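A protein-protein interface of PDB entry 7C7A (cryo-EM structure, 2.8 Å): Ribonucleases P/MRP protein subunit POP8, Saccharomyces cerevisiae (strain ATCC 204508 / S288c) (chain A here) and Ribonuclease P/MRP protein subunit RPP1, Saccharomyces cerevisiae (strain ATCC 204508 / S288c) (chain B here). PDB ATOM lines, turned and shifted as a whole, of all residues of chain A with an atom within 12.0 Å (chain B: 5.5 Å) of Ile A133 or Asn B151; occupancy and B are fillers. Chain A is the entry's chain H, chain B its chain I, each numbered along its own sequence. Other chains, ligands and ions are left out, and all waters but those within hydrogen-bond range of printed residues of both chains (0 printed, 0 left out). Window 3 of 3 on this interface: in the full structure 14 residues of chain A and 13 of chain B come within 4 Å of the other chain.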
ATOM      1  N   GLU A   8     -11.687  -9.517  -0.673  1.00  0.00           N
ATOM      2  CA  GLU A   8     -11.279  -8.788   0.523  1.00  0.00           C
ATOM      3  C   GLU A   8      -9.823  -8.347   0.414  1.00  0.00           C
ATOM      4  O   GLU A   8      -9.513  -7.152   0.481  1.00  0.00           O
ATOM      5  CB  GLU A   8     -11.496  -9.661   1.761  1.00  0.00           C
ATOM      6  CG  GLU A   8     -11.284  -8.947   3.081  1.00  0.00           C
ATOM      7  CD  GLU A   8     -12.351  -7.903   3.354  1.00  0.00           C
ATOM      8  OE1 GLU A   8     -13.475  -8.044   2.826  1.00  0.00           O
ATOM      9  OE2 GLU A   8     -12.070  -6.944   4.101  1.00  0.00           O
ATOM     10  N   GLU A 124     -13.112 -18.937   7.477  1.00  0.00           N
ATOM     11  CA  GLU A 124     -14.476 -19.312   7.097  1.00  0.00           C
ATOM     12  C   GLU A 124     -15.498 -18.952   8.173  1.00  0.00           C
ATOM     13  O   GLU A 124     -16.675 -18.738   7.849  1.00  0.00           O
ATOM     14  CB  GLU A 124     -14.620 -20.796   6.742  1.00  0.00           C
ATOM     15  CG  GLU A 124     -14.134 -21.192   5.346  1.00  0.00           C
ATOM     16  CD  GLU A 124     -12.828 -21.948   5.344  1.00  0.00           C
ATOM     17  OE1 GLU A 124     -12.409 -22.410   6.422  1.00  0.00           O
ATOM     18  OE2 GLU A 124     -12.218 -22.077   4.268  1.00  0.00           O
ATOM     19  N   GLU A 125     -15.098 -18.887   9.449  1.00  0.00           N
ATOM     20  CA  GLU A 125     -16.052 -18.377  10.433  1.00  0.00           C
ATOM     21  C   GLU A 125     -16.296 -16.889  10.221  1.00  0.00           C
ATOM     22  O   GLU A 125     -17.340 -16.372  10.631  1.00  0.00           O
ATOM     23  CB  GLU A 125     -15.589 -18.663  11.868  1.00  0.00           C
ATOM     24  CG  GLU A 125     -14.397 -17.873  12.372  1.00  0.00           C
ATOM     25  CD  GLU A 125     -14.786 -16.570  13.045  1.00  0.00           C
ATOM     26  OE1 GLU A 125     -15.945 -16.445  13.498  1.00  0.00           O
ATOM     27  OE2 GLU A 125     -13.930 -15.663  13.107  1.00  0.00           O
ATOM     28  N   GLU A 126     -15.345 -16.187   9.596  1.00  0.00           N
ATOM     29  CA  GLU A 126     -15.617 -14.849   9.078  1.00  0.00           C
ATOM     30  C   GLU A 126     -16.360 -14.873   7.743  1.00  0.00           C
ATOM     31  O   GLU A 126     -17.135 -13.955   7.458  1.00  0.00           O
ATOM     32  CB  GLU A 126     -14.308 -14.062   8.934  1.00  0.00           C
ATOM     33  CG  GLU A 126     -13.683 -13.658  10.266  1.00  0.00           C
ATOM     34  CD  GLU A 126     -12.393 -12.878  10.099  1.00  0.00           C
ATOM     35  OE1 GLU A 126     -11.899 -12.793   8.957  1.00  0.00           O
ATOM     36  OE2 GLU A 126     -11.881 -12.342  11.106  1.00  0.00           O
ATOM     37  N   GLU A 127     -16.151 -15.912   6.929  1.00  0.00           N
ATOM     38  CA  GLU A 127     -16.817 -16.017   5.636  1.00  0.00           C
ATOM     39  C   GLU A 127     -18.323 -16.168   5.787  1.00  0.00           C
ATOM     40  O   GLU A 127     -19.083 -15.395   5.197  1.00  0.00           O
ATOM     41  CB  GLU A 127     -16.262 -17.204   4.850  1.00  0.00           C
ATOM     42  CG  GLU A 127     -16.900 -17.406   3.486  1.00  0.00           C
ATOM     43  CD  GLU A 127     -16.530 -16.316   2.507  1.00  0.00           C
ATOM     44  OE1 GLU A 127     -15.460 -15.698   2.682  1.00  0.00           O
ATOM     45  OE2 GLU A 127     -17.306 -16.089   1.556  1.00  0.00           O
ATOM     46  N   GLN A 128     -18.769 -17.155   6.561  1.00  0.00           N
ATOM     47  CA  GLN A 128     -20.201 -17.301   6.804  1.00  0.00           C
ATOM     48  C   GLN A 128     -20.760 -16.085   7.533  1.00  0.00           C
ATOM     49  O   GLN A 128     -21.924 -15.711   7.331  1.00  0.00           O
ATOM     50  CB  GLN A 128     -20.481 -18.582   7.587  1.00  0.00           C
ATOM     51  CG  GLN A 128     -20.464 -19.849   6.738  1.00  0.00           C
ATOM     52  CD  GLN A 128     -19.090 -20.173   6.184  1.00  0.00           C
ATOM     53  OE1 GLN A 128     -18.892 -20.215   4.970  1.00  0.00           O
ATOM     54  NE2 GLN A 128     -18.132 -20.401   7.073  1.00  0.00           N
ATOM     55  N   ASP A 129     -19.940 -15.440   8.367  1.00  0.00           N
ATOM     56  CA  ASP A 129     -20.400 -14.259   9.093  1.00  0.00           C
ATOM     57  C   ASP A 129     -20.618 -13.067   8.167  1.00  0.00           C
ATOM     58  O   ASP A 129     -21.529 -12.270   8.399  1.00  0.00           O
ATOM     59  CB  ASP A 129     -19.402 -13.893  10.193  1.00  0.00           C
ATOM     60  CG  ASP A 129     -19.965 -12.888  11.180  1.00  0.00           C
ATOM     61  OD1 ASP A 129     -21.203 -12.800  11.301  1.00  0.00           O
ATOM     62  OD2 ASP A 129     -19.176 -12.181  11.833  1.00  0.00           O
ATOM     63  N   CYS A 130     -19.788 -12.909   7.134  1.00  0.00           N
ATOM     64  CA  CYS A 130     -20.031 -11.836   6.175  1.00  0.00           C
ATOM     65  C   CYS A 130     -21.106 -12.239   5.173  1.00  0.00           C
ATOM     66  O   CYS A 130     -21.762 -11.376   4.576  1.00  0.00           O
ATOM     67  CB  CYS A 130     -18.747 -11.436   5.457  1.00  0.00           C
ATOM     68  SG  CYS A 130     -18.071 -12.681   4.345  1.00  0.00           S
ATOM     69  N   LYS A 131     -21.304 -13.544   4.964  1.00  0.00           N
ATOM     70  CA  LYS A 131     -22.438 -13.975   4.152  1.00  0.00           C
ATOM     71  C   LYS A 131     -23.759 -13.617   4.822  1.00  0.00           C
ATOM     72  O   LYS A 131     -24.653 -13.057   4.175  1.00  0.00           O
ATOM     73  CB  LYS A 131     -22.375 -15.481   3.883  1.00  0.00           C
ATOM     74  CG  LYS A 131     -21.182 -15.977   3.064  1.00  0.00           C
ATOM     75  CD  LYS A 131     -21.254 -15.582   1.589  1.00  0.00           C
ATOM     76  CE  LYS A 131     -20.409 -14.353   1.295  1.00  0.00           C
ATOM     77  NZ  LYS A 131     -20.365 -14.050  -0.160  1.00  0.00           N
ATOM     78  N   CYS A 132     -23.898 -13.923   6.113  1.00  0.00           N
ATOM     79  CA  CYS A 132     -25.143 -13.619   6.812  1.00  0.00           C
ATOM     80  C   CYS A 132     -25.294 -12.119   7.041  1.00  0.00           C
ATOM     81  O   CYS A 132     -26.329 -11.532   6.709  1.00  0.00           O
ATOM     82  CB  CYS A 132     -25.199 -14.376   8.145  1.00  0.00           C
ATOM     83  SG  CYS A 132     -24.039 -13.789   9.398  1.00  0.00           S
ATOM     84  N   ILE A 133     -24.274 -11.484   7.614  1.00  0.00           N
ATOM     85  CA  ILE A 133     -24.315 -10.049   7.878  1.00  0.00           C
ATOM     86  C   ILE A 133     -24.261  -9.270   6.569  1.00  0.00           C
ATOM     87  O   ILE A 133     -25.227  -8.602   6.200  1.00  0.00           O
ATOM     88  CB  ILE A 133     -23.173  -9.613   8.827  1.00  0.00           C
ATOM     89  CG1 ILE A 133     -23.333 -10.272  10.199  1.00  0.00           C
ATOM     90  CG2 ILE A 133     -23.123  -8.098   8.963  1.00  0.00           C
ATOM     91  CD1 ILE A 133     -22.345  -9.778  11.236  1.00  0.00           C
ATOM     92  N   HIS B 143     -15.605  -6.041   8.818  1.00  0.00           N
ATOM     93  CA  HIS B 143     -16.862  -5.952   8.084  1.00  0.00           C
ATOM     94  C   HIS B 143     -18.068  -6.293   8.949  1.00  0.00           C
ATOM     95  O   HIS B 143     -19.182  -5.859   8.639  1.00  0.00           O
ATOM     96  CB  HIS B 143     -16.813  -6.876   6.862  1.00  0.00           C
ATOM     97  CG  HIS B 143     -18.075  -6.891   6.055  1.00  0.00           C
ATOM     98  ND1 HIS B 143     -18.395  -5.902   5.150  1.00  0.00           N
ATOM     99  CD2 HIS B 143     -19.093  -7.783   6.012  1.00  0.00           C
ATOM    100  CE1 HIS B 143     -19.557  -6.182   4.587  1.00  0.00           C
ATOM    101  NE2 HIS B 143     -20.002  -7.318   5.093  1.00  0.00           N
ATOM    102  N   LYS B 144     -17.855  -7.033  10.045  1.00  0.00           N
ATOM    103  CA  LYS B 144     -18.959  -7.539  10.857  1.00  0.00           C
ATOM    104  C   LYS B 144     -19.870  -6.424  11.356  1.00  0.00           C
ATOM    105  O   LYS B 144     -21.077  -6.440  11.086  1.00  0.00           O
ATOM    106  CB  LYS B 144     -18.407  -8.322  12.049  1.00  0.00           C
ATOM    107  CG  LYS B 144     -17.467  -9.456  11.681  1.00  0.00           C
ATOM    108  CD  LYS B 144     -16.844 -10.058  12.931  1.00  0.00           C
ATOM    109  CE  LYS B 144     -15.817 -11.123  12.587  1.00  0.00           C
ATOM    110  NZ  LYS B 144     -16.455 -12.381  12.114  1.00  0.00           N
ATOM    111  N   SER B 145     -19.315  -5.444  12.067  1.00  0.00           N
ATOM    112  CA  SER B 145     -20.100  -4.355  12.641  1.00  0.00           C
ATOM    113  C   SER B 145     -20.319  -3.225  11.639  1.00  0.00           C
ATOM    114  O   SER B 145     -21.348  -2.543  11.678  1.00  0.00           O
ATOM    115  CB  SER B 145     -19.416  -3.833  13.911  1.00  0.00           C
ATOM    116  OG  SER B 145     -18.159  -3.245  13.624  1.00  0.00           O
ATOM    117  N   ILE B 146     -19.363  -3.018  10.733  1.00  0.00           N
ATOM    118  CA  ILE B 146     -19.454  -1.961   9.730  1.00  0.00           C
ATOM    119  C   ILE B 146     -20.628  -2.217   8.792  1.00  0.00           C
ATOM    120  O   ILE B 146     -21.394  -1.299   8.484  1.00  0.00           O
ATOM    121  CB  ILE B 146     -18.134  -1.829   8.947  1.00  0.00           C
ATOM    122  CG1 ILE B 146     -17.060  -1.202   9.835  1.00  0.00           C
ATOM    123  CG2 ILE B 146     -18.331  -0.996   7.691  1.00  0.00           C
ATOM    124  CD1 ILE B 146     -17.424   0.180  10.335  1.00  0.00           C
ATOM    125  N   CYS B 147     -20.787  -3.462   8.334  1.00  0.00           N
ATOM    126  CA  CYS B 147     -21.906  -3.778   7.452  1.00  0.00           C
ATOM    127  C   CYS B 147     -23.240  -3.576   8.161  1.00  0.00           C
ATOM    128  O   CYS B 147     -24.180  -3.014   7.585  1.00  0.00           O
ATOM    129  CB  CYS B 147     -21.784  -5.212   6.940  1.00  0.00           C
ATOM    130  SG  CYS B 147     -23.058  -5.695   5.752  1.00  0.00           S
ATOM    131  N   SER B 148     -23.339  -4.022   9.416  1.00  0.00           N
ATOM    132  CA  SER B 148     -24.579  -3.886  10.169  1.00  0.00           C
ATOM    133  C   SER B 148     -24.897  -2.439  10.520  1.00  0.00           C
ATOM    134  O   SER B 148     -26.074  -2.108  10.699  1.00  0.00           O
ATOM    135  CB  SER B 148     -24.512  -4.726  11.445  1.00  0.00           C
ATOM    136  OG  SER B 148     -23.502  -4.251  12.319  1.00  0.00           O
ATOM    137  N   CYS B 149     -23.888  -1.574  10.630  1.00  0.00           N
ATOM    138  CA  CYS B 149     -24.162  -0.166  10.894  1.00  0.00           C
ATOM    139  C   CYS B 149     -24.384   0.637   9.619  1.00  0.00           C
ATOM    140  O   CYS B 149     -25.000   1.707   9.674  1.00  0.00           O
ATOM    141  CB  CYS B 149     -23.021   0.461  11.703  1.00  0.00           C
ATOM    142  SG  CYS B 149     -21.538   0.871  10.757  1.00  0.00           S
ATOM    143  N   VAL B 150     -23.897   0.153   8.473  1.00  0.00           N
ATOM    144  CA  VAL B 150     -24.141   0.863   7.221  1.00  0.00           C
ATOM    145  C   VAL B 150     -25.483   0.457   6.616  1.00  0.00           C
ATOM    146  O   VAL B 150     -26.161   1.284   5.995  1.00  0.00           O
ATOM    147  CB  VAL B 150     -22.976   0.630   6.240  1.00  0.00           C
ATOM    148  CG1 VAL B 150     -23.312   1.158   4.850  1.00  0.00           C
ATOM    149  CG2 VAL B 150     -21.708   1.297   6.755  1.00  0.00           C
ATOM    150  N   ASN B 151     -25.906  -0.796   6.802  1.00  0.00           N
ATOM    151  CA  ASN B 151     -27.188  -1.236   6.266  1.00  0.00           C
ATOM    152  C   ASN B 151     -28.373  -0.522   6.904  1.00  0.00           C
ATOM    153  O   ASN B 151     -29.436  -0.437   6.279  1.00  0.00           O
ATOM    154  CB  ASN B 151     -27.340  -2.750   6.443  1.00  0.00           C
ATOM    155  CG  ASN B 151     -26.433  -3.537   5.516  1.00  0.00           C
ATOM    156  OD1 ASN B 151     -26.179  -3.129   4.383  1.00  0.00           O
ATOM    157  ND2 ASN B 151     -25.938  -4.672   5.997  1.00  0.00           N
ATOM    158  N   ARG B 152     -28.217  -0.004   8.124  1.00  0.00           N
ATOM    159  CA  ARG B 152     -29.311   0.713   8.769  1.00  0.00           C
ATOM    160  C   ARG B 152     -29.332   2.187   8.372  1.00  0.00           C
ATOM    161  O   ARG B 152     -30.404   2.797   8.311  1.00  0.00           O
ATOM    162  CB  ARG B 152     -29.217   0.571  10.288  1.00  0.00           C
ATOM    163  CG  ARG B 152     -27.812   0.716  10.842  1.00  0.00           C
ATOM    164  CD  ARG B 152     -27.715   0.150  12.248  1.00  0.00           C
ATOM    165  NE  ARG B 152     -28.123   1.119  13.260  1.00  0.00           N
ATOM    166  CZ  ARG B 152     -28.206   0.852  14.559  1.00  0.00           C
ATOM    167  NH1 ARG B 152     -28.587   1.795  15.409  1.00  0.00           N
ATOM    168  NH2 ARG B 152     -27.909  -0.360  15.008  1.00  0.00           N
ATOM    169  N   GLY B 153     -28.167   2.773   8.102  1.00  0.00           N
ATOM    170  CA  GLY B 153     -28.121   4.156   7.666  1.00  0.00           C
ATOM    171  C   GLY B 153     -26.950   4.971   8.180  1.00  0.00           C
ATOM    172  O   GLY B 153     -26.774   6.123   7.771  1.00  0.00           O
ATOM    173  N   ARG B 187     -19.297   2.263   0.258  1.00  0.00           N
ATOM    174  CA  ARG B 187     -20.680   2.676   0.052  1.00  0.00           C
ATOM    175  C   ARG B 187     -21.026   3.915   0.869  1.00  0.00           C
ATOM    176  O   ARG B 187     -21.389   4.957   0.311  1.00  0.00           O
ATOM    177  CB  ARG B 187     -21.632   1.533   0.414  1.00  0.00           C
ATOM    178  CG  ARG B 187     -21.887   0.542  -0.709  1.00  0.00           C
ATOM    179  CD  ARG B 187     -22.880  -0.526  -0.271  1.00  0.00           C
ATOM    180  NE  ARG B 187     -23.466  -1.236  -1.404  1.00  0.00           N
ATOM    181  CZ  ARG B 187     -24.493  -2.073  -1.309  1.00  0.00           C
ATOM    182  NH1 ARG B 187     -25.052  -2.309  -0.130  1.00  0.00           N
ATOM    183  NH2 ARG B 187     -24.962  -2.675  -2.394  1.00  0.00           N
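The side-chain amino group of Lys B144 is in salt-bridge range of the side-chain carboxylate of Asp A129 (2.7 Å).
The backbone carbonyl oxygen (O) of Ile A133 is in hydrogen-bond range of the side-chain sulfur (SG) of Cys B147, at 3.7 Å.
O of Glu A126 lies within hydrogen-bond range of SG of Cys A130, 3.5 Å away.
O of Glu A127 lies within hydrogen-bond range of SG of Cys A130, at 3.0 Å.
O of Asp A129 is in hydrogen-bond range of SG of Cys A132 (3.1 Å).
NE2 of His B143 sits close to SG of Cys B147, 3.5 Å away.
The backbone carbonyl oxygen (O) of Lys B144 is in hydrogen-bond range of the side-chain hydroxyl (OG) of Ser B148 (3.5 Å).
ND2 of Asn B151 lies within hydrogen-bond range of O of Cys B147 (2.9 Å).
NZ of Lys B144 touches CG of Glu A126 (3.6 Å).
Cys A130 touches His B143 (CB to CD2, 3.7 Å).
CG2 of Ile A133 touches O of Lys B144, at 3.4 Å.
Ile A133 touches Asn B151 (O to ND2, 3.999 Å).
Of the printed residues of chain B, Ile A133 touches Lys B144, Cys B147 and Asn B151.
Printed residues of chain A within 4 Å of Asn B151: Ile A133.
Of the printed residues of chain A, His B143 touches Cys A130.
Cys B147 touches one residue of chain A.
No residue of chain A comes within 4 Å of Ser B148.
No residue of chain A comes within 4 Å of Cys B149.
No residue of chain A comes within 4 Å of Val B150.
No residue of chain A comes within 4 Å of Gly B153.
Printed residues of chain B within 4 Å of Cys A130: His B143.
Printed residues of chain B within 4 Å of Glu A126: Lys B144 (3.6 Å).
Printed residues of chain B within 4 Å of Asp A129: Lys B144.
Gln A128 touches none of the printed residues of chain B.
Cys A132 touches none of the printed residues of chain B.
The nearest printed residue of chain A that does not touch Asn B151 is Cys A132 (6.9 Å).
The nearest printed residue of chain B that does not touch Asp A129 is His B143 (5.6 Å).
Of the 12 printed residues of chain B, 4 touch a printed residue of chain A.
Of the 11 printed residues of chain A, 4 touch a printed residue of chain B.
Hydrophobic or aromatic side chains of chain A that line the printed part of chain B: Ile A133.
Among the printed residues, 6 pairs touch across the chains.
Among the printed residues, Asp or Glu carboxylates within 4 Å of a Lys or Arg side-chain nitrogen of the other chain: Asp A129 with Lys B144 (2.7 Å).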
